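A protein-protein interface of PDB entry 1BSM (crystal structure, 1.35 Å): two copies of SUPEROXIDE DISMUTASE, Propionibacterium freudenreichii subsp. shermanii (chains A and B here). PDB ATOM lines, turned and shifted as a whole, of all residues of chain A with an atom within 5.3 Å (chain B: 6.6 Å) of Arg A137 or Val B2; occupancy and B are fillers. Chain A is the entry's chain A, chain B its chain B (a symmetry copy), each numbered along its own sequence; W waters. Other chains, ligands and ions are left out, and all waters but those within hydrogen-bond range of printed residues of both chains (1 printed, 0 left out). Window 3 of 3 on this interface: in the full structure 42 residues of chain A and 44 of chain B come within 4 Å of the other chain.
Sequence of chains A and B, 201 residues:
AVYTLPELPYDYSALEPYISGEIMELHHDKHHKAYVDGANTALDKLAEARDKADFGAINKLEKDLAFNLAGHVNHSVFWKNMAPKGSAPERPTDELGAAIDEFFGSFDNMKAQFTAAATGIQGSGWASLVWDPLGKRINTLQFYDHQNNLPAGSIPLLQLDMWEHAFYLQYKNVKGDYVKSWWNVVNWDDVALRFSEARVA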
ATOM      1  N   PHE A 103       7.160  -0.351 -29.058  1.00  0.00           N
ATOM      2  CA  PHE A 103       6.790   0.739 -28.163  1.00  0.00           C
ATOM      3  C   PHE A 103       7.169   2.152 -28.591  1.00  0.00           C
ATOM      4  O   PHE A 103       6.783   3.121 -27.933  1.00  0.00           O
ATOM      5  CB  PHE A 103       7.296   0.436 -26.752  1.00  0.00           C
ATOM      6  CG  PHE A 103       6.778  -0.862 -26.202  1.00  0.00           C
ATOM      7  CD1 PHE A 103       5.413  -1.048 -25.999  1.00  0.00           C
ATOM      8  CD2 PHE A 103       7.645  -1.916 -25.926  1.00  0.00           C
ATOM      9  CE1 PHE A 103       4.916  -2.266 -25.537  1.00  0.00           C
ATOM     10  CE2 PHE A 103       7.155  -3.140 -25.464  1.00  0.00           C
ATOM     11  CZ  PHE A 103       5.788  -3.312 -25.268  1.00  0.00           C
ATOM     12  N   VAL A 130      13.446   2.712 -19.718  1.00  0.00           N
ATOM     13  CA  VAL A 130      13.135   1.723 -18.690  1.00  0.00           C
ATOM     14  C   VAL A 130      12.064   0.713 -19.073  1.00  0.00           C
ATOM     15  O   VAL A 130      11.325   0.897 -20.041  1.00  0.00           O
ATOM     16  CB  VAL A 130      12.638   2.414 -17.391  1.00  0.00           C
ATOM     17  CG1 VAL A 130      13.670   3.398 -16.876  1.00  0.00           C
ATOM     18  CG2 VAL A 130      11.301   3.116 -17.647  1.00  0.00           C
ATOM     19  N   TRP A 131      11.998  -0.365 -18.298  1.00  0.00           N
ATOM     20  CA  TRP A 131      10.982  -1.383 -18.497  1.00  0.00           C
ATOM     21  C   TRP A 131       9.923  -1.127 -17.432  1.00  0.00           C
ATOM     22  O   TRP A 131      10.230  -1.030 -16.241  1.00  0.00           O
ATOM     23  CB  TRP A 131      11.548  -2.797 -18.337  1.00  0.00           C
ATOM     24  CG  TRP A 131      10.476  -3.869 -18.371  1.00  0.00           C
ATOM     25  CD1 TRP A 131       9.980  -4.569 -17.305  1.00  0.00           C
ATOM     26  CD2 TRP A 131       9.765  -4.344 -19.522  1.00  0.00           C
ATOM     27  NE1 TRP A 131       9.008  -5.444 -17.723  1.00  0.00           N
ATOM     28  CE2 TRP A 131       8.854  -5.329 -19.077  1.00  0.00           C
ATOM     29  CE3 TRP A 131       9.810  -4.034 -20.890  1.00  0.00           C
ATOM     30  CZ2 TRP A 131       7.997  -6.006 -19.949  1.00  0.00           C
ATOM     31  CZ3 TRP A 131       8.952  -4.708 -21.757  1.00  0.00           C
ATOM     32  CH2 TRP A 131       8.058  -5.683 -21.280  1.00  0.00           C
ATOM     33  N   ASP A 132       8.697  -0.931 -17.894  1.00  0.00           N
ATOM     34  CA  ASP A 132       7.540  -0.692 -17.045  1.00  0.00           C
ATOM     35  C   ASP A 132       6.908  -2.068 -16.808  1.00  0.00           C
ATOM     36  O   ASP A 132       6.310  -2.644 -17.714  1.00  0.00           O
ATOM     37  CB  ASP A 132       6.580   0.254 -17.786  1.00  0.00           C
ATOM     38  CG  ASP A 132       5.201   0.348 -17.150  1.00  0.00           C
ATOM     39  OD1 ASP A 132       5.010  -0.064 -15.985  1.00  0.00           O
ATOM     40  OD2 ASP A 132       4.295   0.849 -17.844  1.00  0.00           O
ATOM     41  N   PRO A 133       7.058  -2.615 -15.590  1.00  0.00           N
ATOM     42  CA  PRO A 133       6.508  -3.930 -15.239  1.00  0.00           C
ATOM     43  C   PRO A 133       4.984  -3.989 -15.126  1.00  0.00           C
ATOM     44  O   PRO A 133       4.394  -5.063 -15.252  1.00  0.00           O
ATOM     45  CB  PRO A 133       7.191  -4.233 -13.907  1.00  0.00           C
ATOM     46  CG  PRO A 133       7.299  -2.888 -13.283  1.00  0.00           C
ATOM     47  CD  PRO A 133       7.752  -2.014 -14.437  1.00  0.00           C
ATOM     48  N   GLY A 135       2.752  -1.871 -16.985  1.00  0.00           N
ATOM     49  CA  GLY A 135       2.232  -1.775 -18.335  1.00  0.00           C
ATOM     50  C   GLY A 135       2.878  -2.781 -19.272  1.00  0.00           C
ATOM     51  O   GLY A 135       2.424  -2.950 -20.404  1.00  0.00           O
ATOM     52  N   LYS A 136       3.924  -3.456 -18.792  1.00  0.00           N
ATOM     53  CA  LYS A 136       4.664  -4.449 -19.575  1.00  0.00           C
ATOM     54  C   LYS A 136       5.122  -3.830 -20.894  1.00  0.00           C
ATOM     55  O   LYS A 136       4.803  -4.323 -21.978  1.00  0.00           O
ATOM     56  CB  LYS A 136       3.801  -5.695 -19.823  1.00  0.00           C
ATOM     57  CG  LYS A 136       3.365  -6.415 -18.549  1.00  0.00           C
ATOM     58  CD  LYS A 136       4.562  -6.881 -17.723  1.00  0.00           C
ATOM     59  CE  LYS A 136       5.301  -8.034 -18.388  1.00  0.00           C
ATOM     60  NZ  LYS A 136       6.575  -8.363 -17.686  1.00  0.00           N
ATOM     61  N   ARG A 137       5.904  -2.760 -20.784  1.00  0.00           N
ATOM     62  CA  ARG A 137       6.380  -2.032 -21.954  1.00  0.00           C
ATOM     63  C   ARG A 137       7.663  -1.256 -21.680  1.00  0.00           C
ATOM     64  O   ARG A 137       8.120  -1.181 -20.544  1.00  0.00           O
ATOM     65  CB  ARG A 137       5.298  -1.042 -22.385  1.00  0.00           C
ATOM     66  CG  ARG A 137       4.866  -0.092 -21.270  1.00  0.00           C
ATOM     67  CD  ARG A 137       3.741   0.830 -21.713  1.00  0.00           C
ATOM     68  NE  ARG A 137       4.160   1.695 -22.813  1.00  0.00           N
ATOM     69  CZ  ARG A 137       3.562   1.756 -23.998  1.00  0.00           C
ATOM     70  NH1 ARG A 137       2.503   0.997 -24.259  1.00  0.00           N
ATOM     71  NH2 ARG A 137       4.032   2.573 -24.929  1.00  0.00           N
ATOM     72  N   ILE A 138       8.252  -0.703 -22.737  1.00  0.00           N
ATOM     73  CA  ILE A 138       9.458   0.107 -22.606  1.00  0.00           C
ATOM     74  C   ILE A 138       9.039   1.568 -22.752  1.00  0.00           C
ATOM     75  O   ILE A 138       8.369   1.937 -23.720  1.00  0.00           O
ATOM     76  CB  ILE A 138      10.515  -0.212 -23.695  1.00  0.00           C
ATOM     77  CG1 ILE A 138      10.967  -1.671 -23.605  1.00  0.00           C
ATOM     78  CG2 ILE A 138      11.723   0.708 -23.534  1.00  0.00           C
ATOM     79  CD1 ILE A 138      12.035  -2.041 -24.619  1.00  0.00           C
ATOM     80  N   ASN A 139       9.410   2.383 -21.769  1.00  0.00           N
ATOM     81  CA  ASN A 139       9.097   3.810 -21.770  1.00  0.00           C
ATOM     82  C   ASN A 139      10.375   4.613 -21.571  1.00  0.00           C
ATOM     83  O   ASN A 139      11.421   4.062 -21.233  1.00  0.00           O
ATOM     84  CB  ASN A 139       8.170   4.165 -20.597  1.00  0.00           C
ATOM     85  CG  ASN A 139       6.776   3.589 -20.730  1.00  0.00           C
ATOM     86  OD1 ASN A 139       6.149   3.240 -19.727  1.00  0.00           O
ATOM     87  ND2 ASN A 139       6.261   3.534 -21.951  1.00  0.00           N
ATOM     88  N   ALA B   1      -7.023  -0.431 -23.417  1.00  0.00           N
ATOM     89  CA  ALA B   1      -6.060   0.587 -22.908  1.00  0.00           C
ATOM     90  C   ALA B   1      -4.848  -0.091 -22.277  1.00  0.00           C
ATOM     91  O   ALA B   1      -4.924  -1.246 -21.852  1.00  0.00           O
ATOM     92  CB  ALA B   1      -6.745   1.500 -21.894  1.00  0.00           C
ATOM     93  N   VAL B   2      -3.729   0.627 -22.223  1.00  0.00           N
ATOM     94  CA  VAL B   2      -2.507   0.085 -21.636  1.00  0.00           C
ATOM     95  C   VAL B   2      -2.647  -0.137 -20.126  1.00  0.00           C
ATOM     96  O   VAL B   2      -2.205  -1.160 -19.605  1.00  0.00           O
ATOM     97  CB  VAL B   2      -1.264   0.970 -21.973  1.00  0.00           C
ATOM     98  CG1 VAL B   2      -1.569   2.431 -21.742  1.00  0.00           C
ATOM     99  CG2 VAL B   2      -0.050   0.546 -21.151  1.00  0.00           C
ATOM    100  N   TYR B   3      -3.300   0.796 -19.438  1.00  0.00           N
ATOM    101  CA  TYR B   3      -3.499   0.685 -17.994  1.00  0.00           C
ATOM    102  C   TYR B   3      -4.977   0.578 -17.642  1.00  0.00           C
ATOM    103  O   TYR B   3      -5.823   1.188 -18.295  1.00  0.00           O
ATOM    104  CB  TYR B   3      -2.898   1.890 -17.263  1.00  0.00           C
ATOM    105  CG  TYR B   3      -1.427   2.095 -17.527  1.00  0.00           C
ATOM    106  CD1 TYR B   3      -0.478   1.189 -17.052  1.00  0.00           C
ATOM    107  CD2 TYR B   3      -0.983   3.189 -18.266  1.00  0.00           C
ATOM    108  CE1 TYR B   3       0.877   1.369 -17.314  1.00  0.00           C
ATOM    109  CE2 TYR B   3       0.365   3.378 -18.532  1.00  0.00           C
ATOM    110  CZ  TYR B   3       1.291   2.467 -18.054  1.00  0.00           C
ATOM    111  OH  TYR B   3       2.625   2.652 -18.327  1.00  0.00           O
ATOM    112  N   THR B   4      -5.274  -0.199 -16.603  1.00  0.00           N
ATOM    113  CA  THR B   4      -6.644  -0.393 -16.142  1.00  0.00           C
ATOM    114  C   THR B   4      -6.712  -0.281 -14.619  1.00  0.00           C
ATOM    115  O   THR B   4      -5.722  -0.512 -13.922  1.00  0.00           O
ATOM    116  CB  THR B   4      -7.200  -1.772 -16.591  1.00  0.00           C
ATOM    117  OG1 THR B   4      -7.136  -1.871 -18.018  1.00  0.00           O
ATOM    118  CG2 THR B   4      -8.649  -1.931 -16.173  1.00  0.00           C
ATOM    119  N   ALA B  39      -2.202   8.258 -16.872  1.00  0.00           N
ATOM    120  CA  ALA B  39      -1.093   7.466 -17.392  1.00  0.00           C
ATOM    121  C   ALA B  39      -1.371   7.060 -18.840  1.00  0.00           C
ATOM    122  O   ALA B  39      -0.469   7.081 -19.681  1.00  0.00           O
ATOM    123  CB  ALA B  39      -0.869   6.241 -16.524  1.00  0.00           C
ATOM    124  N   ASN B  40      -2.621   6.697 -19.127  1.00  0.00           N
ATOM    125  CA  ASN B  40      -3.013   6.316 -20.485  1.00  0.00           C
ATOM    126  C   ASN B  40      -2.874   7.522 -21.413  1.00  0.00           C
ATOM    127  O   ASN B  40      -2.363   7.408 -22.527  1.00  0.00           O
ATOM    128  CB  ASN B  40      -4.461   5.812 -20.520  1.00  0.00           C
ATOM    129  CG  ASN B  40      -4.603   4.389 -20.002  1.00  0.00           C
ATOM    130  OD1 ASN B  40      -3.709   3.559 -20.174  1.00  0.00           O
ATOM    131  ND2 ASN B  40      -5.741   4.098 -19.380  1.00  0.00           N
ATOM    132  N   THR B  41      -3.327   8.680 -20.938  1.00  0.00           N
ATOM    133  CA  THR B  41      -3.255   9.911 -21.715  1.00  0.00           C
ATOM    134  C   THR B  41      -1.815  10.328 -21.995  1.00  0.00           C
ATOM    135  O   THR B  41      -1.501  10.748 -23.107  1.00  0.00           O
ATOM    136  CB  THR B  41      -4.006  11.055 -21.015  1.00  0.00           C
ATOM    137  OG1 THR B  41      -5.400  10.730 -20.952  1.00  0.00           O
ATOM    138  CG2 THR B  41      -3.834  12.371 -21.770  1.00  0.00           C
ATOM    139  N   LEU B  43       0.858   8.442 -22.293  1.00  0.00           N
ATOM    140  CA  LEU B  43       1.413   7.582 -23.331  1.00  0.00           C
ATOM    141  C   LEU B  43       0.847   7.936 -24.704  1.00  0.00           C
ATOM    142  O   LEU B  43       1.578   7.951 -25.692  1.00  0.00           O
ATOM    143  CB  LEU B  43       1.156   6.108 -23.023  1.00  0.00           C
ATOM    144  CG  LEU B  43       1.958   5.486 -21.879  1.00  0.00           C
ATOM    145  CD1 LEU B  43       1.612   4.011 -21.763  1.00  0.00           C
ATOM    146  CD2 LEU B  43       3.453   5.649 -22.137  1.00  0.00           C
ATOM    147  N   ASP B  44      -0.451   8.226 -24.760  1.00  0.00           N
ATOM    148  CA  ASP B  44      -1.095   8.596 -26.019  1.00  0.00           C
ATOM    149  C   ASP B  44      -0.476   9.869 -26.585  1.00  0.00           C
ATOM    150  O   ASP B  44      -0.252   9.981 -27.790  1.00  0.00           O
ATOM    151  CB  ASP B  44      -2.601   8.804 -25.822  1.00  0.00           C
ATOM    152  CG  ASP B  44      -3.355   7.502 -25.594  1.00  0.00           C
ATOM    153  OD1 ASP B  44      -2.840   6.428 -25.972  1.00  0.00           O
ATOM    154  OD2 ASP B  44      -4.473   7.558 -25.041  1.00  0.00           O
ATOM    155  N   ARG B  50       5.752  11.483 -31.200  1.00  0.00           N
ATOM    156  CA  ARG B  50       6.637  10.705 -32.066  1.00  0.00           C
ATOM    157  C   ARG B  50       6.204  10.741 -33.530  1.00  0.00           C
ATOM    158  O   ARG B  50       7.029  10.933 -34.423  1.00  0.00           O
ATOM    159  CB  ARG B  50       6.719   9.251 -31.587  1.00  0.00           C
ATOM    160  CG  ARG B  50       7.685   9.032 -30.434  1.00  0.00           C
ATOM    161  CD  ARG B  50       7.826   7.562 -30.069  1.00  0.00           C
ATOM    162  NE  ARG B  50       6.848   7.126 -29.072  1.00  0.00           N
ATOM    163  CZ  ARG B  50       5.815   6.328 -29.327  1.00  0.00           C
ATOM    164  NH1 ARG B  50       5.604   5.874 -30.555  1.00  0.00           N
ATOM    165  NH2 ARG B  50       5.005   5.963 -28.342  1.00  0.00           N
ATOM    166  N   HIS B  72      -0.433   5.104 -10.121  1.00  0.00           N
ATOM    167  CA  HIS B  72      -1.092   3.847 -10.452  1.00  0.00           C
ATOM    168  C   HIS B  72      -0.374   2.683  -9.762  1.00  0.00           C
ATOM    169  O   HIS B  72      -1.012   1.820  -9.158  1.00  0.00           O
ATOM    170  CB  HIS B  72      -1.098   3.657 -11.973  1.00  0.00           C
ATOM    171  CG  HIS B  72      -1.810   2.420 -12.433  1.00  0.00           C
ATOM    172  ND1 HIS B  72      -1.634   1.890 -13.692  1.00  0.00           N
ATOM    173  CD2 HIS B  72      -2.695   1.612 -11.804  1.00  0.00           C
ATOM    174  CE1 HIS B  72      -2.377   0.806 -13.818  1.00  0.00           C
ATOM    175  NE2 HIS B  72      -3.030   0.615 -12.687  1.00  0.00           N
HETATM  176  O   HOH W   1      -0.615  -2.885 -20.945  1.00  0.00           O
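Of the 11 printed residues of chain B, 4 touch a printed residue of chain A.
Printed residues of chain A that touch a printed residue of chain B: Phe A103, Asp A132, Gly A135, Arg A137 and Asn A139.
Among the printed residues, no Asp or Glu carboxylate lies within 4 Å of a Lys or Arg side-chain nitrogen of the other chain.
The guanidinium group of Arg B50 is in hydrogen-bond range of the backbone carbonyl oxygen of Phe A103 (3.4 Å).
The side-chain carboxylate (OD2) of Asp A132 lies within hydrogen-bond range of the side-chain hydroxyl (OH) of Tyr B3, at 2.5 Å.
No position is printed for both chains.
Val B2 touches just one residue of chain A: Arg A137 (3.8 Å).
Of the printed residues of chain B, Gly A135 touches Tyr B3.
Of the printed residues of chain A, Leu B43 touches Arg A137 and Asn A139.
Ala B39 touches none of the printed residues of chain A.
Among the printed residues, merely in contact across the chains: Asn A139 with Leu B43, Gly A135 with Tyr B3, Arg A137 with Leu B43, Asn A139 with Tyr B3 and Arg A137 with Val B2.
The backbone carbonyl oxygen of Asn A139 sits at hydrogen-bond distance from the backbone NH of Val A130, at 2.9 Å.
The side-chain carboxylate (OD1) of Asp A132 lies within hydrogen-bond range of the backbone NH (N) of Gly A135 (3.1 Å).
N of Asp A132 sits at hydrogen-bond distance from O of Arg A137.
NE of Arg A137 sits close to ND2 of Asn A139, 2.9 Å away.
The backbone NH (N) of Tyr B3 is in hydrogen-bond range of the side-chain amide oxygen (OD1) of Asn B40, 2.9 Å away.
Water W1 bridges O of Val B2 (2.7 Å) and O of Gly A135 (3.1 Å).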
